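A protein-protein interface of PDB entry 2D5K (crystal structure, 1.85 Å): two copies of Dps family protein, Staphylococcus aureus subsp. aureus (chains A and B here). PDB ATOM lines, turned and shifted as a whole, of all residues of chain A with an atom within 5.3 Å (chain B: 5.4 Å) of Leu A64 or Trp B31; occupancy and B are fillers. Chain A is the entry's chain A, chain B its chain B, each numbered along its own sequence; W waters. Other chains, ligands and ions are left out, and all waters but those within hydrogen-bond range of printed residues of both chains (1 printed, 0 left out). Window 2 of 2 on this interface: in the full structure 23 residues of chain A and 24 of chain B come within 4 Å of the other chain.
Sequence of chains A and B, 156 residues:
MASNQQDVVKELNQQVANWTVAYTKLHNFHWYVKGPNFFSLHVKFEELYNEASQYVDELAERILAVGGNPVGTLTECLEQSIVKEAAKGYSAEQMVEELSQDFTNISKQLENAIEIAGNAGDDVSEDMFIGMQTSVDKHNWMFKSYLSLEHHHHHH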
ATOM      1  N   VAL A  16      27.540  18.196  18.637  1.00  0.00           N
ATOM      2  CA  VAL A  16      27.261  19.328  19.519  1.00  0.00           C
ATOM      3  C   VAL A  16      26.201  18.862  20.517  1.00  0.00           C
ATOM      4  O   VAL A  16      26.291  19.134  21.717  1.00  0.00           O
ATOM      5  CB  VAL A  16      26.726  20.552  18.734  1.00  0.00           C
ATOM      6  CG1 VAL A  16      26.218  21.620  19.706  1.00  0.00           C
ATOM      7  CG2 VAL A  16      27.833  21.136  17.870  1.00  0.00           C
ATOM      8  N   VAL A  56      32.144  21.296  22.059  1.00  0.00           N
ATOM      9  CA  VAL A  56      30.884  21.932  21.720  1.00  0.00           C
ATOM     10  C   VAL A  56      31.119  23.258  21.010  1.00  0.00           C
ATOM     11  O   VAL A  56      30.538  23.513  19.957  1.00  0.00           O
ATOM     12  CB  VAL A  56      30.021  22.168  22.980  1.00  0.00           C
ATOM     13  CG1 VAL A  56      28.886  23.141  22.670  1.00  0.00           C
ATOM     14  CG2 VAL A  56      29.452  20.833  23.468  1.00  0.00           C
ATOM     15  N   ASP A  57      31.980  24.095  21.574  1.00  0.00           N
ATOM     16  CA  ASP A  57      32.247  25.388  20.960  1.00  0.00           C
ATOM     17  C   ASP A  57      32.973  25.250  19.622  1.00  0.00           C
ATOM     18  O   ASP A  57      32.641  25.942  18.660  1.00  0.00           O
ATOM     19  CB  ASP A  57      33.059  26.271  21.907  1.00  0.00           C
ATOM     20  CG  ASP A  57      33.078  27.723  21.469  1.00  0.00           C
ATOM     21  OD1 ASP A  57      31.986  28.279  21.216  1.00  0.00           O
ATOM     22  OD2 ASP A  57      34.176  28.308  21.385  1.00  0.00           O
ATOM     23  N   LEU A  59      33.057  22.647  17.387  1.00  0.00           N
ATOM     24  CA  LEU A  59      32.212  22.123  16.325  1.00  0.00           C
ATOM     25  C   LEU A  59      31.082  23.078  15.958  1.00  0.00           C
ATOM     26  O   LEU A  59      30.712  23.197  14.787  1.00  0.00           O
ATOM     27  CB  LEU A  59      31.652  20.756  16.728  1.00  0.00           C
ATOM     28  CG  LEU A  59      32.719  19.689  17.006  1.00  0.00           C
ATOM     29  CD1 LEU A  59      32.052  18.331  17.111  1.00  0.00           C
ATOM     30  CD2 LEU A  59      33.758  19.673  15.895  1.00  0.00           C
ATOM     31  N   ALA A  60      30.542  23.774  16.952  1.00  0.00           N
ATOM     32  CA  ALA A  60      29.464  24.717  16.690  1.00  0.00           C
ATOM     33  C   ALA A  60      29.961  25.863  15.817  1.00  0.00           C
ATOM     34  O   ALA A  60      29.257  26.309  14.910  1.00  0.00           O
ATOM     35  CB  ALA A  60      28.910  25.263  17.999  1.00  0.00           C
ATOM     36  N   GLU A  61      31.175  26.338  16.080  1.00  0.00           N
ATOM     37  CA  GLU A  61      31.704  27.437  15.285  1.00  0.00           C
ATOM     38  C   GLU A  61      32.169  26.970  13.908  1.00  0.00           C
ATOM     39  O   GLU A  61      32.337  27.779  12.998  1.00  0.00           O
ATOM     40  CB  GLU A  61      32.814  28.168  16.052  1.00  0.00           C
ATOM     41  CG  GLU A  61      32.308  28.717  17.394  1.00  0.00           C
ATOM     42  CD  GLU A  61      33.143  29.859  17.951  1.00  0.00           C
ATOM     43  OE1 GLU A  61      34.375  29.859  17.758  1.00  0.00           O
ATOM     44  OE2 GLU A  61      32.557  30.751  18.604  1.00  0.00           O
ATOM     45  N   ARG A  62      32.368  25.664  13.744  1.00  0.00           N
ATOM     46  CA  ARG A  62      32.743  25.153  12.430  1.00  0.00           C
ATOM     47  C   ARG A  62      31.455  25.186  11.610  1.00  0.00           C
ATOM     48  O   ARG A  62      31.466  25.535  10.427  1.00  0.00           O
ATOM     49  CB  ARG A  62      33.279  23.721  12.504  1.00  0.00           C
ATOM     50  CG  ARG A  62      33.518  23.080  11.125  1.00  0.00           C
ATOM     51  CD  ARG A  62      34.426  23.937  10.224  1.00  0.00           C
ATOM     52  NE  ARG A  62      34.526  23.395   8.865  1.00  0.00           N
ATOM     53  CZ  ARG A  62      34.990  24.073   7.815  1.00  0.00           C
ATOM     54  NH1 ARG A  62      35.403  25.325   7.959  1.00  0.00           N
ATOM     55  NH2 ARG A  62      35.023  23.508   6.612  1.00  0.00           N
ATOM     56  N   ILE A  63      30.340  24.828  12.245  1.00  0.00           N
ATOM     57  CA  ILE A  63      29.049  24.859  11.561  1.00  0.00           C
ATOM     58  C   ILE A  63      28.801  26.286  11.074  1.00  0.00           C
ATOM     59  O   ILE A  63      28.370  26.507   9.938  1.00  0.00           O
ATOM     60  CB  ILE A  63      27.894  24.430  12.501  1.00  0.00           C
ATOM     61  CG1 ILE A  63      28.008  22.936  12.808  1.00  0.00           C
ATOM     62  CG2 ILE A  63      26.543  24.713  11.842  1.00  0.00           C
ATOM     63  CD1 ILE A  63      26.938  22.416  13.759  1.00  0.00           C
ATOM     64  N   LEU A  64      29.086  27.256  11.935  1.00  0.00           N
ATOM     65  CA  LEU A  64      28.899  28.654  11.574  1.00  0.00           C
ATOM     66  C   LEU A  64      29.807  29.019  10.406  1.00  0.00           C
ATOM     67  O   LEU A  64      29.407  29.763   9.507  1.00  0.00           O
ATOM     68  CB  LEU A  64      29.208  29.557  12.775  1.00  0.00           C
ATOM     69  CG  LEU A  64      28.244  29.440  13.960  1.00  0.00           C
ATOM     70  CD1 LEU A  64      28.852  30.103  15.180  1.00  0.00           C
ATOM     71  CD2 LEU A  64      26.905  30.083  13.606  1.00  0.00           C
ATOM     72  N   ALA A  65      31.023  28.479  10.419  1.00  0.00           N
ATOM     73  CA  ALA A  65      32.009  28.751   9.377  1.00  0.00           C
ATOM     74  C   ALA A  65      31.626  28.198   8.007  1.00  0.00           C
ATOM     75  O   ALA A  65      32.203  28.600   6.998  1.00  0.00           O
ATOM     76  CB  ALA A  65      33.381  28.206   9.797  1.00  0.00           C
ATOM     77  N   VAL A  66      30.673  27.269   7.963  1.00  0.00           N
ATOM     78  CA  VAL A  66      30.237  26.725   6.681  1.00  0.00           C
ATOM     79  C   VAL A  66      28.822  27.192   6.352  1.00  0.00           C
ATOM     80  O   VAL A  66      28.168  26.658   5.454  1.00  0.00           O
ATOM     81  CB  VAL A  66      30.292  25.178   6.647  1.00  0.00           C
ATOM     82  CG1 VAL A  66      31.718  24.712   6.915  1.00  0.00           C
ATOM     83  CG2 VAL A  66      29.325  24.584   7.656  1.00  0.00           C
ATOM     84  N   GLY A  67      28.357  28.194   7.093  1.00  0.00           N
ATOM     85  CA  GLY A  67      27.040  28.753   6.854  1.00  0.00           C
ATOM     86  C   GLY A  67      25.857  28.036   7.472  1.00  0.00           C
ATOM     87  O   GLY A  67      24.712  28.311   7.102  1.00  0.00           O
ATOM     88  N   GLY A  68      26.114  27.132   8.414  1.00  0.00           N
ATOM     89  CA  GLY A  68      25.028  26.400   9.046  1.00  0.00           C
ATOM     90  C   GLY A  68      24.552  26.977  10.369  1.00  0.00           C
ATOM     91  O   GLY A  68      25.067  27.995  10.840  1.00  0.00           O
ATOM     92  N   PRO A  70      24.151  26.036  14.298  1.00  0.00           N
ATOM     93  CA  PRO A  70      24.467  25.086  15.374  1.00  0.00           C
ATOM     94  C   PRO A  70      23.265  24.943  16.301  1.00  0.00           C
ATOM     95  O   PRO A  70      22.596  25.933  16.592  1.00  0.00           O
ATOM     96  CB  PRO A  70      25.638  25.747  16.108  1.00  0.00           C
ATOM     97  CG  PRO A  70      26.147  26.796  15.155  1.00  0.00           C
ATOM     98  CD  PRO A  70      24.925  27.278  14.444  1.00  0.00           C
ATOM     99  N   VAL A  71      22.989  23.729  16.771  1.00  0.00           N
ATOM    100  CA  VAL A  71      21.864  23.526  17.682  1.00  0.00           C
ATOM    101  C   VAL A  71      22.132  24.326  18.955  1.00  0.00           C
ATOM    102  O   VAL A  71      23.079  24.044  19.695  1.00  0.00           O
ATOM    103  CB  VAL A  71      21.666  22.028  18.019  1.00  0.00           C
ATOM    104  CG1 VAL A  71      21.131  21.298  16.800  1.00  0.00           C
ATOM    105  CG2 VAL A  71      22.978  21.406  18.462  1.00  0.00           C
ATOM    106  N   GLY A  72      21.289  25.325  19.203  1.00  0.00           N
ATOM    107  CA  GLY A  72      21.482  26.185  20.357  1.00  0.00           C
ATOM    108  C   GLY A  72      20.462  26.168  21.481  1.00  0.00           C
ATOM    109  O   GLY A  72      20.308  27.167  22.180  1.00  0.00           O
ATOM    110  N   LEU B  26      23.611  31.260  26.559  1.00  0.00           N
ATOM    111  CA  LEU B  26      24.762  32.130  26.351  1.00  0.00           C
ATOM    112  C   LEU B  26      25.641  31.601  25.220  1.00  0.00           C
ATOM    113  O   LEU B  26      26.309  32.376  24.548  1.00  0.00           O
ATOM    114  CB  LEU B  26      25.568  32.280  27.645  1.00  0.00           C
ATOM    115  CG  LEU B  26      24.919  33.204  28.680  1.00  0.00           C
ATOM    116  CD1 LEU B  26      25.545  32.979  30.051  1.00  0.00           C
ATOM    117  CD2 LEU B  26      25.086  34.653  28.244  1.00  0.00           C
ATOM    118  N   HIS B  27      25.651  30.285  25.012  1.00  0.00           N
ATOM    119  CA  HIS B  27      26.422  29.720  23.910  1.00  0.00           C
ATOM    120  C   HIS B  27      25.718  30.128  22.623  1.00  0.00           C
ATOM    121  O   HIS B  27      26.355  30.507  21.643  1.00  0.00           O
ATOM    122  CB  HIS B  27      26.478  28.191  23.987  1.00  0.00           C
ATOM    123  CG  HIS B  27      27.635  27.671  24.778  1.00  0.00           C
ATOM    124  ND1 HIS B  27      27.680  27.721  26.155  1.00  0.00           N
ATOM    125  CD2 HIS B  27      28.805  27.113  24.382  1.00  0.00           C
ATOM    126  CE1 HIS B  27      28.828  27.214  26.573  1.00  0.00           C
ATOM    127  NE2 HIS B  27      29.528  26.838  25.517  1.00  0.00           N
ATOM    128  N   ASN B  28      24.391  30.046  22.643  1.00  0.00           N
ATOM    129  CA  ASN B  28      23.579  30.417  21.490  1.00  0.00           C
ATOM    130  C   ASN B  28      23.880  31.862  21.095  1.00  0.00           C
ATOM    131  O   ASN B  28      24.153  32.153  19.928  1.00  0.00           O
ATOM    132  CB  ASN B  28      22.094  30.251  21.837  1.00  0.00           C
ATOM    133  CG  ASN B  28      21.173  30.627  20.690  1.00  0.00           C
ATOM    134  OD1 ASN B  28      21.172  31.768  20.230  1.00  0.00           O
ATOM    135  ND2 ASN B  28      20.377  29.664  20.224  1.00  0.00           N
ATOM    136  N   PHE B  29      23.846  32.771  22.066  1.00  0.00           N
ATOM    137  CA  PHE B  29      24.117  34.176  21.777  1.00  0.00           C
ATOM    138  C   PHE B  29      25.564  34.356  21.319  1.00  0.00           C
ATOM    139  O   PHE B  29      25.850  35.154  20.431  1.00  0.00           O
ATOM    140  CB  PHE B  29      23.819  35.043  23.008  1.00  0.00           C
ATOM    141  CG  PHE B  29      22.345  35.154  23.338  1.00  0.00           C
ATOM    142  CD1 PHE B  29      21.385  34.528  22.541  1.00  0.00           C
ATOM    143  CD2 PHE B  29      21.921  35.884  24.445  1.00  0.00           C
ATOM    144  CE1 PHE B  29      20.024  34.628  22.843  1.00  0.00           C
ATOM    145  CE2 PHE B  29      20.563  35.991  24.755  1.00  0.00           C
ATOM    146  CZ  PHE B  29      19.613  35.360  23.949  1.00  0.00           C
ATOM    147  N   HIS B  30      26.466  33.598  21.933  1.00  0.00           N
ATOM    148  CA  HIS B  30      27.890  33.620  21.605  1.00  0.00           C
ATOM    149  C   HIS B  30      28.088  33.249  20.130  1.00  0.00           C
ATOM    150  O   HIS B  30      28.921  33.832  19.436  1.00  0.00           O
ATOM    151  CB  HIS B  30      28.601  32.621  22.536  1.00  0.00           C
ATOM    152  CG  HIS B  30      30.011  32.282  22.152  1.00  0.00           C
ATOM    153  ND1 HIS B  30      31.057  33.172  22.270  1.00  0.00           N
ATOM    154  CD2 HIS B  30      30.562  31.108  21.756  1.00  0.00           C
ATOM    155  CE1 HIS B  30      32.191  32.561  21.970  1.00  0.00           C
ATOM    156  NE2 HIS B  30      31.917  31.309  21.655  1.00  0.00           N
ATOM    157  N   TRP B  31      27.298  32.293  19.647  1.00  0.00           N
ATOM    158  CA  TRP B  31      27.413  31.836  18.265  1.00  0.00           C
ATOM    159  C   TRP B  31      26.654  32.671  17.245  1.00  0.00           C
ATOM    160  O   TRP B  31      27.159  32.944  16.155  1.00  0.00           O
ATOM    161  CB  TRP B  31      26.917  30.387  18.136  1.00  0.00           C
ATOM    162  CG  TRP B  31      27.673  29.391  18.965  1.00  0.00           C
ATOM    163  CD1 TRP B  31      29.007  29.405  19.251  1.00  0.00           C
ATOM    164  CD2 TRP B  31      27.140  28.215  19.589  1.00  0.00           C
ATOM    165  NE1 TRP B  31      29.339  28.312  20.020  1.00  0.00           N
ATOM    166  CE2 TRP B  31      28.213  27.564  20.239  1.00  0.00           C
ATOM    167  CE3 TRP B  31      25.861  27.647  19.659  1.00  0.00           C
ATOM    168  CZ2 TRP B  31      28.046  26.372  20.956  1.00  0.00           C
ATOM    169  CZ3 TRP B  31      25.692  26.457  20.374  1.00  0.00           C
ATOM    170  CH2 TRP B  31      26.783  25.836  21.012  1.00  0.00           C
ATOM    171  N   TYR B  32      25.438  33.065  17.602  1.00  0.00           N
ATOM    172  CA  TYR B  32      24.570  33.798  16.689  1.00  0.00           C
ATOM    173  C   TYR B  32      24.612  35.320  16.683  1.00  0.00           C
ATOM    174  O   TYR B  32      23.957  35.945  15.847  1.00  0.00           O
ATOM    175  CB  TYR B  32      23.128  33.333  16.911  1.00  0.00           C
ATOM    176  CG  TYR B  32      22.865  31.920  16.436  1.00  0.00           C
ATOM    177  CD1 TYR B  32      22.796  31.625  15.075  1.00  0.00           C
ATOM    178  CD2 TYR B  32      22.679  30.876  17.346  1.00  0.00           C
ATOM    179  CE1 TYR B  32      22.543  30.329  14.626  1.00  0.00           C
ATOM    180  CE2 TYR B  32      22.427  29.574  16.908  1.00  0.00           C
ATOM    181  CZ  TYR B  32      22.358  29.311  15.543  1.00  0.00           C
ATOM    182  OH  TYR B  32      22.088  28.036  15.098  1.00  0.00           O
ATOM    183  N   VAL B  33      25.365  35.923  17.599  1.00  0.00           N
ATOM    184  CA  VAL B  33      25.433  37.379  17.645  1.00  0.00           C
ATOM    185  C   VAL B  33      26.004  37.935  16.344  1.00  0.00           C
ATOM    186  O   VAL B  33      26.932  37.369  15.763  1.00  0.00           O
ATOM    187  CB  VAL B  33      26.286  37.870  18.844  1.00  0.00           C
ATOM    188  CG1 VAL B  33      27.759  37.531  18.628  1.00  0.00           C
ATOM    189  CG2 VAL B  33      26.093  39.373  19.039  1.00  0.00           C
ATOM    190  N   LYS B  34      25.430  39.039  15.875  1.00  0.00           N
ATOM    191  CA  LYS B  34      25.880  39.659  14.637  1.00  0.00           C
ATOM    192  C   LYS B  34      25.904  41.177  14.752  1.00  0.00           C
ATOM    193  O   LYS B  34      25.352  41.745  15.692  1.00  0.00           O
ATOM    194  CB  LYS B  34      24.969  39.239  13.483  1.00  0.00           C
ATOM    195  CG  LYS B  34      24.964  37.734  13.247  1.00  0.00           C
ATOM    196  CD  LYS B  34      24.127  37.341  12.051  1.00  0.00           C
ATOM    197  CE  LYS B  34      24.071  35.829  11.913  1.00  0.00           C
ATOM    198  NZ  LYS B  34      25.433  35.214  11.878  1.00  0.00           N
ATOM    199  N   PHE B  38      30.086  42.588  17.203  1.00  0.00           N
ATOM    200  CA  PHE B  38      30.345  41.154  17.246  1.00  0.00           C
ATOM    201  C   PHE B  38      31.530  40.741  18.107  1.00  0.00           C
ATOM    202  O   PHE B  38      31.410  39.873  18.967  1.00  0.00           O
ATOM    203  CB  PHE B  38      30.588  40.595  15.843  1.00  0.00           C
ATOM    204  CG  PHE B  38      31.006  39.152  15.844  1.00  0.00           C
ATOM    205  CD1 PHE B  38      30.056  38.138  15.927  1.00  0.00           C
ATOM    206  CD2 PHE B  38      32.357  38.805  15.850  1.00  0.00           C
ATOM    207  CE1 PHE B  38      30.442  36.801  16.021  1.00  0.00           C
ATOM    208  CE2 PHE B  38      32.755  37.471  15.944  1.00  0.00           C
ATOM    209  CZ  PHE B  38      31.795  36.467  16.032  1.00  0.00           C
ATOM    210  N   HIS B  42      30.771  38.643  21.391  1.00  0.00           N
ATOM    211  CA  HIS B  42      31.135  37.241  21.205  1.00  0.00           C
ATOM    212  C   HIS B  42      31.960  36.803  22.417  1.00  0.00           C
ATOM    213  O   HIS B  42      31.727  35.739  22.995  1.00  0.00           O
ATOM    214  CB  HIS B  42      31.939  37.085  19.904  1.00  0.00           C
ATOM    215  CG  HIS B  42      32.421  35.692  19.643  1.00  0.00           C
ATOM    216  ND1 HIS B  42      33.759  35.359  19.631  1.00  0.00           N
ATOM    217  CD2 HIS B  42      31.747  34.552  19.366  1.00  0.00           C
ATOM    218  CE1 HIS B  42      33.888  34.073  19.357  1.00  0.00           C
ATOM    219  NE2 HIS B  42      32.682  33.560  19.192  1.00  0.00           N
HETATM  220  O   HOH W   1      34.806  30.753  21.339  1.00  0.00           O
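The side-chain carboxylate (OD1) of Asp A57 lies within hydrogen-bond range of a ring nitrogen (NE2) of His B30, at 3.1 Å. OD1 of Asp A57 is in hydrogen-bond range of NE1 of Trp B31 (2.9 Å). The side-chain carboxylate (OE2) of Glu A61 lies within hydrogen-bond range of a ring nitrogen (NE2) of His B30, at 3.2 Å. A ring nitrogen (NE2) of His B42 is in hydrogen-bond range of the side-chain carboxylate (OE2) of Glu A61. O of Pro A70 is in hydrogen-bond range of OH of Tyr B32, 2.6 Å away. The side-chain amide nitrogen of Asn B28 sits at hydrogen-bond distance from the backbone carbonyl oxygen of Gly A72 (3.2 Å).
Of the 11 printed residues of chain B, 5 touch a printed residue of chain A. Hydrophobic or aromatic side chains of chain B within 4 Å of the printed part of chain A: His B30, Trp B31, Tyr B32 and His B42. Of the 16 printed residues of chain A, 8 touch a printed residue of chain B. Among the printed residues, no Asp or Glu carboxylate lies within 4 Å of a Lys or Arg side-chain nitrogen of the other chain.
No position is printed for both chains. Of the 11 pairs that touch across the chains among the printed residues, none has its exchanged pair printed and touching as well.
Among the printed residues, pairs that only touch across the chains: Ala A60 with Trp B31, Leu A64 with Trp B31, Val A71 with Trp B31, Val A56 with Trp B31 and Glu A61 with Trp B31.
Printed residues of chain B within 4 Å of Asp A57: His B30 and Trp B31. Of the printed residues of chain B, Ala A60 touches Trp B31 (3.3 Å). Leu A64 touches one residue of chain B. Printed residues of chain B within 4 Å of Val A71: Trp B31. Printed residues of chain B within 4 Å of Gly A72: Asn B28. Phe B29 touches none of the printed residues of chain A. Of the printed residues of chain A, Trp B31 touches Val A56, Asp A57, Ala A60, Glu A61, Leu A64 and Val A71. The nearest printed residue of chain B that does not touch Pro A70 is Trp B31 (4.03 Å).
Water W1 lies within hydrogen-bond range of OD2 of Asp A57 (2.5 Å) and NE2 of His B30 (3.0 Å).
A ring nitrogen (ND1) of His B30 lies within hydrogen-bond range of the backbone carbonyl oxygen (O) of His B42 (2.8 Å).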
